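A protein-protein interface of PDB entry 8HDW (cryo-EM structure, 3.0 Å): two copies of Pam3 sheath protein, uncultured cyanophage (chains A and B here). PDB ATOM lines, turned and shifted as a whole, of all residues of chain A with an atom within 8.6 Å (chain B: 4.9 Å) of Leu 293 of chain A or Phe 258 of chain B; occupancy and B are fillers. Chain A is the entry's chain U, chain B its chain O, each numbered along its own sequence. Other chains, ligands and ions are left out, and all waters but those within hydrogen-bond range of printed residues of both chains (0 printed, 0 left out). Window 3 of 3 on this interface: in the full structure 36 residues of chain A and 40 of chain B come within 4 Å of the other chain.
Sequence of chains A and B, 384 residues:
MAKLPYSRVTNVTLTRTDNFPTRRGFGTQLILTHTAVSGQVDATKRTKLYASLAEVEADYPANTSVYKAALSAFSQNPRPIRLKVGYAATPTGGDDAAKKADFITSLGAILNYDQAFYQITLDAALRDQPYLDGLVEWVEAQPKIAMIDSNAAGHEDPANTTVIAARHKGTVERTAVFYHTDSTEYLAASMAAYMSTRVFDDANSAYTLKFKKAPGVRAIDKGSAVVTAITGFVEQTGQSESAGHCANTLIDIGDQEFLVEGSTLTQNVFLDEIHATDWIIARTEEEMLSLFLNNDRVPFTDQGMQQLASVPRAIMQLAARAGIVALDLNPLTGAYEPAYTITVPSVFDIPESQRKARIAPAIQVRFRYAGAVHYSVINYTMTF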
ATOM      1  N   GLU A 286     -11.444  15.396  24.461  1.00  0.00           N
ATOM      2  CA  GLU A 286     -10.324  14.876  23.688  1.00  0.00           C
ATOM      3  C   GLU A 286      -9.056  15.669  23.957  1.00  0.00           C
ATOM      4  O   GLU A 286      -7.970  15.094  24.087  1.00  0.00           O
ATOM      5  CB  GLU A 286     -10.672  14.897  22.202  1.00  0.00           C
ATOM      6  CG  GLU A 286     -10.135  13.715  21.413  1.00  0.00           C
ATOM      7  CD  GLU A 286      -8.622  13.737  21.260  1.00  0.00           C
ATOM      8  OE1 GLU A 286      -8.036  14.837  21.225  1.00  0.00           O
ATOM      9  OE2 GLU A 286      -8.015  12.648  21.172  1.00  0.00           O
ATOM     10  N   GLU A 287      -9.172  16.993  24.048  1.00  0.00           N
ATOM     11  CA  GLU A 287      -7.992  17.808  24.319  1.00  0.00           C
ATOM     12  C   GLU A 287      -7.477  17.597  25.739  1.00  0.00           C
ATOM     13  O   GLU A 287      -6.261  17.582  25.965  1.00  0.00           O
ATOM     14  CB  GLU A 287      -8.300  19.278  24.056  1.00  0.00           C
ATOM     15  CG  GLU A 287      -8.429  19.618  22.582  1.00  0.00           C
ATOM     16  CD  GLU A 287      -7.089  19.654  21.856  1.00  0.00           C
ATOM     17  OE1 GLU A 287      -6.101  20.152  22.436  1.00  0.00           O
ATOM     18  OE2 GLU A 287      -7.024  19.189  20.698  1.00  0.00           O
ATOM     19  N   MET A 288      -8.373  17.415  26.712  1.00  0.00           N
ATOM     20  CA  MET A 288      -7.919  17.092  28.059  1.00  0.00           C
ATOM     21  C   MET A 288      -7.157  15.779  28.081  1.00  0.00           C
ATOM     22  O   MET A 288      -6.095  15.682  28.703  1.00  0.00           O
ATOM     23  CB  MET A 288      -9.097  17.020  29.028  1.00  0.00           C
ATOM     24  CG  MET A 288      -9.715  18.352  29.381  1.00  0.00           C
ATOM     25  SD  MET A 288      -8.611  19.421  30.310  1.00  0.00           S
ATOM     26  CE  MET A 288      -8.079  18.290  31.578  1.00  0.00           C
ATOM     27  N   LEU A 289      -7.682  14.751  27.410  1.00  0.00           N
ATOM     28  CA  LEU A 289      -6.981  13.471  27.379  1.00  0.00           C
ATOM     29  C   LEU A 289      -5.636  13.597  26.676  1.00  0.00           C
ATOM     30  O   LEU A 289      -4.641  13.016  27.119  1.00  0.00           O
ATOM     31  CB  LEU A 289      -7.842  12.413  26.695  1.00  0.00           C
ATOM     32  CG  LEU A 289      -7.797  10.979  27.226  1.00  0.00           C
ATOM     33  CD1 LEU A 289      -7.852   9.990  26.077  1.00  0.00           C
ATOM     34  CD2 LEU A 289      -6.584  10.714  28.098  1.00  0.00           C
ATOM     35  N   SER A 290      -5.583  14.341  25.587  1.00  0.00           N
ATOM     36  CA  SER A 290      -4.312  14.557  24.907  1.00  0.00           C
ATOM     37  C   SER A 290      -3.325  15.365  25.740  1.00  0.00           C
ATOM     38  O   SER A 290      -2.122  15.278  25.514  1.00  0.00           O
ATOM     39  CB  SER A 290      -4.560  15.244  23.566  1.00  0.00           C
ATOM     40  OG  SER A 290      -3.389  15.267  22.774  1.00  0.00           O
ATOM     41  N   LEU A 291      -3.786  16.164  26.697  1.00  0.00           N
ATOM     42  CA  LEU A 291      -2.896  16.813  27.650  1.00  0.00           C
ATOM     43  C   LEU A 291      -2.344  15.869  28.707  1.00  0.00           C
ATOM     44  O   LEU A 291      -1.208  16.046  29.140  1.00  0.00           O
ATOM     45  CB  LEU A 291      -3.619  17.967  28.354  1.00  0.00           C
ATOM     46  CG  LEU A 291      -2.830  18.832  29.334  1.00  0.00           C
ATOM     47  CD1 LEU A 291      -2.009  19.854  28.587  1.00  0.00           C
ATOM     48  CD2 LEU A 291      -3.760  19.513  30.310  1.00  0.00           C
ATOM     49  N   PHE A 292      -3.119  14.876  29.136  1.00  0.00           N
ATOM     50  CA  PHE A 292      -2.643  13.939  30.146  1.00  0.00           C
ATOM     51  C   PHE A 292      -1.658  12.924  29.587  1.00  0.00           C
ATOM     52  O   PHE A 292      -0.933  12.298  30.364  1.00  0.00           O
ATOM     53  CB  PHE A 292      -3.822  13.201  30.779  1.00  0.00           C
ATOM     54  CG  PHE A 292      -4.485  13.951  31.893  1.00  0.00           C
ATOM     55  CD1 PHE A 292      -3.741  14.685  32.794  1.00  0.00           C
ATOM     56  CD2 PHE A 292      -5.860  13.914  32.041  1.00  0.00           C
ATOM     57  CE1 PHE A 292      -4.354  15.365  33.821  1.00  0.00           C
ATOM     58  CE2 PHE A 292      -6.479  14.595  33.063  1.00  0.00           C
ATOM     59  CZ  PHE A 292      -5.726  15.321  33.953  1.00  0.00           C
ATOM     60  N   LEU A 293      -1.614  12.741  28.269  1.00  0.00           N
ATOM     61  CA  LEU A 293      -0.720  11.761  27.666  1.00  0.00           C
ATOM     62  C   LEU A 293       0.619  12.351  27.242  1.00  0.00           C
ATOM     63  O   LEU A 293       1.599  11.609  27.127  1.00  0.00           O
ATOM     64  CB  LEU A 293      -1.388  11.114  26.451  1.00  0.00           C
ATOM     65  CG  LEU A 293      -2.683  10.325  26.649  1.00  0.00           C
ATOM     66  CD1 LEU A 293      -3.345  10.083  25.310  1.00  0.00           C
ATOM     67  CD2 LEU A 293      -2.429   9.014  27.343  1.00  0.00           C
ATOM     68  N   ASN A 294       0.689  13.660  27.004  1.00  0.00           N
ATOM     69  CA  ASN A 294       1.949  14.279  26.598  1.00  0.00           C
ATOM     70  C   ASN A 294       2.846  14.563  27.796  1.00  0.00           C
ATOM     71  O   ASN A 294       4.032  14.221  27.796  1.00  0.00           O
ATOM     72  CB  ASN A 294       1.682  15.570  25.824  1.00  0.00           C
ATOM     73  CG  ASN A 294       1.183  15.316  24.425  1.00  0.00           C
ATOM     74  OD1 ASN A 294       0.692  14.231  24.115  1.00  0.00           O
ATOM     75  ND2 ASN A 294       1.306  16.320  23.567  1.00  0.00           N
ATOM     76  N   ASN A 295       2.300  15.206  28.818  1.00  0.00           N
ATOM     77  CA  ASN A 295       3.097  15.605  29.964  1.00  0.00           C
ATOM     78  C   ASN A 295       3.545  14.400  30.771  1.00  0.00           C
ATOM     79  O   ASN A 295       2.890  13.356  30.787  1.00  0.00           O
ATOM     80  CB  ASN A 295       2.302  16.538  30.867  1.00  0.00           C
ATOM     81  CG  ASN A 295       1.946  17.814  30.189  1.00  0.00           C
ATOM     82  OD1 ASN A 295       2.758  18.731  30.100  1.00  0.00           O
ATOM     83  ND2 ASN A 295       0.715  17.898  29.710  1.00  0.00           N
ATOM     84  N   ASP A 296       4.686  14.551  31.442  1.00  0.00           N
ATOM     85  CA  ASP A 296       5.036  13.606  32.492  1.00  0.00           C
ATOM     86  C   ASP A 296       3.930  13.562  33.531  1.00  0.00           C
ATOM     87  O   ASP A 296       3.229  12.558  33.649  1.00  0.00           O
ATOM     88  CB  ASP A 296       6.374  13.981  33.129  1.00  0.00           C
ATOM     89  CG  ASP A 296       6.497  15.470  33.403  1.00  0.00           C
ATOM     90  OD1 ASP A 296       6.095  16.269  32.530  1.00  0.00           O
ATOM     91  OD2 ASP A 296       6.991  15.839  34.495  1.00  0.00           O
ATOM     92  N   ARG A 297       3.707  14.678  34.231  1.00  0.00           N
ATOM     93  CA  ARG A 297       2.604  14.849  35.165  1.00  0.00           C
ATOM     94  C   ARG A 297       1.964  16.216  34.997  1.00  0.00           C
ATOM     95  O   ARG A 297       2.494  17.089  34.308  1.00  0.00           O
ATOM     96  CB  ARG A 297       3.043  14.727  36.609  1.00  0.00           C
ATOM     97  CG  ARG A 297       3.525  13.383  36.936  1.00  0.00           C
ATOM     98  CD  ARG A 297       2.585  12.334  36.405  1.00  0.00           C
ATOM     99  NE  ARG A 297       3.283  11.096  36.055  1.00  0.00           N
ATOM    100  CZ  ARG A 297       2.852  10.194  35.177  1.00  0.00           C
ATOM    101  NH1 ARG A 297       1.715  10.385  34.521  1.00  0.00           N
ATOM    102  NH2 ARG A 297       3.572   9.106  34.940  1.00  0.00           N
ATOM    103  N   VAL A 298       0.814  16.383  35.639  1.00  0.00           N
ATOM    104  CA  VAL A 298       0.184  17.678  35.860  1.00  0.00           C
ATOM    105  C   VAL A 298       0.141  17.907  37.369  1.00  0.00           C
ATOM    106  O   VAL A 298      -0.619  17.230  38.074  1.00  0.00           O
ATOM    107  CB  VAL A 298      -1.217  17.749  35.238  1.00  0.00           C
ATOM    108  CG1 VAL A 298      -1.853  19.092  35.520  1.00  0.00           C
ATOM    109  CG2 VAL A 298      -1.132  17.528  33.749  1.00  0.00           C
ATOM    110  N   PHE B 211      -0.034   7.248  35.699  1.00  0.00           N
ATOM    111  CA  PHE B 211      -1.466   7.023  35.579  1.00  0.00           C
ATOM    112  C   PHE B 211      -1.967   7.036  34.146  1.00  0.00           C
ATOM    113  O   PHE B 211      -3.017   6.450  33.879  1.00  0.00           O
ATOM    114  CB  PHE B 211      -2.215   8.076  36.409  1.00  0.00           C
ATOM    115  CG  PHE B 211      -3.717   8.038  36.280  1.00  0.00           C
ATOM    116  CD1 PHE B 211      -4.418   6.864  36.363  1.00  0.00           C
ATOM    117  CD2 PHE B 211      -4.428   9.207  36.139  1.00  0.00           C
ATOM    118  CE1 PHE B 211      -5.793   6.857  36.253  1.00  0.00           C
ATOM    119  CE2 PHE B 211      -5.798   9.196  36.033  1.00  0.00           C
ATOM    120  CZ  PHE B 211      -6.478   8.020  36.096  1.00  0.00           C
ATOM    121  N   LYS B 212      -1.278   7.697  33.218  1.00  0.00           N
ATOM    122  CA  LYS B 212      -1.617   7.579  31.799  1.00  0.00           C
ATOM    123  C   LYS B 212      -0.333   7.361  31.007  1.00  0.00           C
ATOM    124  O   LYS B 212       0.197   8.297  30.406  1.00  0.00           O
ATOM    125  CB  LYS B 212      -2.385   8.804  31.305  1.00  0.00           C
ATOM    126  CG  LYS B 212      -2.210  10.069  32.125  1.00  0.00           C
ATOM    127  CD  LYS B 212      -3.307  10.251  33.168  1.00  0.00           C
ATOM    128  CE  LYS B 212      -4.656   9.723  32.703  1.00  0.00           C
ATOM    129  NZ  LYS B 212      -5.174  10.407  31.496  1.00  0.00           N
ATOM    130  N   LYS B 213       0.124   6.112  30.954  1.00  0.00           N
ATOM    131  CA  LYS B 213       1.399   5.779  30.338  1.00  0.00           C
ATOM    132  C   LYS B 213       1.231   4.558  29.445  1.00  0.00           C
ATOM    133  O   LYS B 213       0.635   3.559  29.851  1.00  0.00           O
ATOM    134  CB  LYS B 213       2.469   5.516  31.401  1.00  0.00           C
ATOM    135  CG  LYS B 213       2.895   6.751  32.153  1.00  0.00           C
ATOM    136  CD  LYS B 213       3.618   7.700  31.232  1.00  0.00           C
ATOM    137  CE  LYS B 213       3.868   9.038  31.894  1.00  0.00           C
ATOM    138  NZ  LYS B 213       2.631   9.830  32.039  1.00  0.00           N
ATOM    139  N   ALA B 214       1.770   4.646  28.235  1.00  0.00           N
ATOM    140  CA  ALA B 214       1.679   3.678  27.152  1.00  0.00           C
ATOM    141  C   ALA B 214       2.860   2.718  27.171  1.00  0.00           C
ATOM    142  O   ALA B 214       4.012   3.155  27.135  1.00  0.00           O
ATOM    143  CB  ALA B 214       1.633   4.392  25.802  1.00  0.00           C
ATOM    144  N   LEU B 250      -4.998  -1.197  31.939  1.00  0.00           N
ATOM    145  CA  LEU B 250      -4.638  -0.686  30.613  1.00  0.00           C
ATOM    146  C   LEU B 250      -5.869  -0.558  29.708  1.00  0.00           C
ATOM    147  O   LEU B 250      -6.055  -1.302  28.750  1.00  0.00           O
ATOM    148  CB  LEU B 250      -3.577  -1.568  29.947  1.00  0.00           C
ATOM    149  CG  LEU B 250      -2.970  -0.955  28.691  1.00  0.00           C
ATOM    150  CD1 LEU B 250      -1.672  -0.268  29.024  1.00  0.00           C
ATOM    151  CD2 LEU B 250      -2.766  -2.001  27.632  1.00  0.00           C
ATOM    152  N   ILE B 251      -6.721   0.398  30.059  1.00  0.00           N
ATOM    153  CA  ILE B 251      -7.919   0.702  29.284  1.00  0.00           C
ATOM    154  C   ILE B 251      -7.561   1.481  28.025  1.00  0.00           C
ATOM    155  O   ILE B 251      -6.424   1.933  27.861  1.00  0.00           O
ATOM    156  CB  ILE B 251      -8.922   1.491  30.133  1.00  0.00           C
ATOM    157  CG1 ILE B 251      -8.480   2.946  30.229  1.00  0.00           C
ATOM    158  CG2 ILE B 251      -9.020   0.881  31.511  1.00  0.00           C
ATOM    159  CD1 ILE B 251      -9.451   3.826  30.948  1.00  0.00           C
ATOM    160  N   ILE B 253      -9.531   4.675  25.703  1.00  0.00           N
ATOM    161  CA  ILE B 253     -10.650   5.610  25.687  1.00  0.00           C
ATOM    162  C   ILE B 253     -10.863   6.207  24.304  1.00  0.00           C
ATOM    163  O   ILE B 253     -11.929   6.042  23.702  1.00  0.00           O
ATOM    164  CB  ILE B 253     -10.470   6.723  26.740  1.00  0.00           C
ATOM    165  CG1 ILE B 253     -10.614   6.144  28.144  1.00  0.00           C
ATOM    166  CG2 ILE B 253     -11.480   7.823  26.520  1.00  0.00           C
ATOM    167  CD1 ILE B 253     -10.692   7.188  29.229  1.00  0.00           C
ATOM    168  N   GLN B 256      -6.255   5.896  21.830  1.00  0.00           N
ATOM    169  CA  GLN B 256      -5.038   5.645  22.592  1.00  0.00           C
ATOM    170  C   GLN B 256      -5.306   4.577  23.641  1.00  0.00           C
ATOM    171  O   GLN B 256      -6.419   4.470  24.162  1.00  0.00           O
ATOM    172  CB  GLN B 256      -4.542   6.925  23.254  1.00  0.00           C
ATOM    173  CG  GLN B 256      -4.219   8.048  22.296  1.00  0.00           C
ATOM    174  CD  GLN B 256      -5.403   8.942  22.049  1.00  0.00           C
ATOM    175  OE1 GLN B 256      -6.517   8.642  22.474  1.00  0.00           O
ATOM    176  NE2 GLN B 256      -5.172  10.054  21.365  1.00  0.00           N
ATOM    177  N   GLU B 257      -4.281   3.792  23.950  1.00  0.00           N
ATOM    178  CA  GLU B 257      -4.314   2.834  25.044  1.00  0.00           C
ATOM    179  C   GLU B 257      -3.277   3.246  26.080  1.00  0.00           C
ATOM    180  O   GLU B 257      -2.153   3.609  25.722  1.00  0.00           O
ATOM    181  CB  GLU B 257      -4.033   1.426  24.526  1.00  0.00           C
ATOM    182  CG  GLU B 257      -3.318   1.429  23.187  1.00  0.00           C
ATOM    183  CD  GLU B 257      -3.058   0.037  22.657  1.00  0.00           C
ATOM    184  OE1 GLU B 257      -3.686  -0.920  23.162  1.00  0.00           O
ATOM    185  OE2 GLU B 257      -2.223  -0.100  21.741  1.00  0.00           O
ATOM    186  N   PHE B 258      -3.658   3.203  27.355  1.00  0.00           N
ATOM    187  CA  PHE B 258      -2.771   3.667  28.409  1.00  0.00           C
ATOM    188  C   PHE B 258      -3.146   3.006  29.724  1.00  0.00           C
ATOM    189  O   PHE B 258      -4.274   2.552  29.915  1.00  0.00           O
ATOM    190  CB  PHE B 258      -2.806   5.196  28.537  1.00  0.00           C
ATOM    191  CG  PHE B 258      -4.182   5.769  28.734  1.00  0.00           C
ATOM    192  CD1 PHE B 258      -4.698   5.948  30.001  1.00  0.00           C
ATOM    193  CD2 PHE B 258      -4.947   6.154  27.652  1.00  0.00           C
ATOM    194  CE1 PHE B 258      -5.953   6.480  30.181  1.00  0.00           C
ATOM    195  CE2 PHE B 258      -6.198   6.686  27.831  1.00  0.00           C
ATOM    196  CZ  PHE B 258      -6.700   6.848  29.096  1.00  0.00           C
ATOM    197  N   LEU B 259      -2.174   2.953  30.630  1.00  0.00           N
ATOM    198  CA  LEU B 259      -2.396   2.373  31.947  1.00  0.00           C
ATOM    199  C   LEU B 259      -3.380   3.234  32.724  1.00  0.00           C
ATOM    200  O   LEU B 259      -3.521   4.427  32.464  1.00  0.00           O
ATOM    201  CB  LEU B 259      -1.072   2.259  32.700  1.00  0.00           C
ATOM    202  CG  LEU B 259      -1.013   1.439  33.985  1.00  0.00           C
ATOM    203  CD1 LEU B 259       0.159   0.495  33.925  1.00  0.00           C
ATOM    204  CD2 LEU B 259      -0.877   2.350  35.180  1.00  0.00           C
ATOM    205  N   VAL B 260      -4.101   2.618  33.658  1.00  0.00           N
ATOM    206  CA  VAL B 260      -5.107   3.348  34.412  1.00  0.00           C
ATOM    207  C   VAL B 260      -5.036   2.969  35.884  1.00  0.00           C
ATOM    208  O   VAL B 260      -4.543   1.905  36.260  1.00  0.00           O
ATOM    209  CB  VAL B 260      -6.532   3.125  33.860  1.00  0.00           C
ATOM    210  CG1 VAL B 260      -7.185   1.922  34.505  1.00  0.00           C
ATOM    211  CG2 VAL B 260      -7.374   4.366  34.059  1.00  0.00           C
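N of Phe 258 of chain B is in hydrogen-bond range of O of Ile 251 of chain B, at 3.1 Å.
O of Phe 211 of chain B lies close to O of Leu 259 of chain B.
The backbone carbonyl oxygen (O) of Lys 213 of chain B sits at hydrogen-bond distance from the backbone NH (N) of Leu 259 of chain B (3.0 Å).
The backbone carbonyl oxygen of Leu 291 of chain A is in hydrogen-bond range of the side-chain amide nitrogen of Asn 295 of chain A (2.7 Å).
No position is printed for both chains.
Hydrophobic or aromatic side chains of chain B within 4 Å of the printed part of chain A: Phe 258.
Of the 13 printed residues of chain A, 7 touch a printed residue of chain B.
Hydrophobic or aromatic side chains of chain A that line the printed part of chain B: Leu 289, Phe 292 and Leu 293.
Among the printed residues, 11 pairs touch across the chains.
Among the printed residues, no Asp or Glu carboxylate lies within 4 Å of a Lys or Arg side-chain nitrogen of the other chain.
OE2 of Glu 286 of chain A touches NE2 of Gln 256 of chain B, at 3.9 Å.
Lys 212 of chain B touches Leu 289 of chain A (NZ to CD2, 3.7 Å).
CD2 of Leu 289 of chain A touches CZ of Phe 258 of chain B (3.99 Å).
Phe 292 of chain A touches Lys 212 of chain B (O to CG, 3.1 Å).
CD2 of Leu 293 of chain A touches CB of Lys 212 of chain B, 3.97 Å away.
Gln 256 of chain B touches Leu 293 of chain A (CG to CD1, 3.7 Å).
Leu 293 of chain A touches Phe 258 of chain B (CD2 to CD2, 3.8 Å).
Lys 213 of chain B touches Asn 295 of chain A.
Phe 211 of chain B touches Arg 297 of chain A (N to NH1, 3.8 Å).
NZ of Lys 213 of chain B lies within hydrogen-bond range of O of Asp 296 of chain A (3.2 Å).
The side-chain amino group of Lys 213 of chain B lies close to the guanidinium group of Arg 297 of chain A, at 2.7 Å.
Met 288 of chain A touches none of the printed residues of chain B.
Printed residues of chain B within 4 Å of Leu 289 of chain A: Lys 212 (3.7 Å) and Phe 258 (3.99 Å).
Leu 293 of chain A touches just these residues of chain B: Lys 212, Gln 256 and Phe 258.
Printed residues of chain B within 4 Å of Asp 296 of chain A: Lys 213 (3.2 Å).
Of the printed residues of chain A, Phe 211 of chain B touches Arg 297.
Leu 250 of chain B touches none of the printed residues of chain A.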
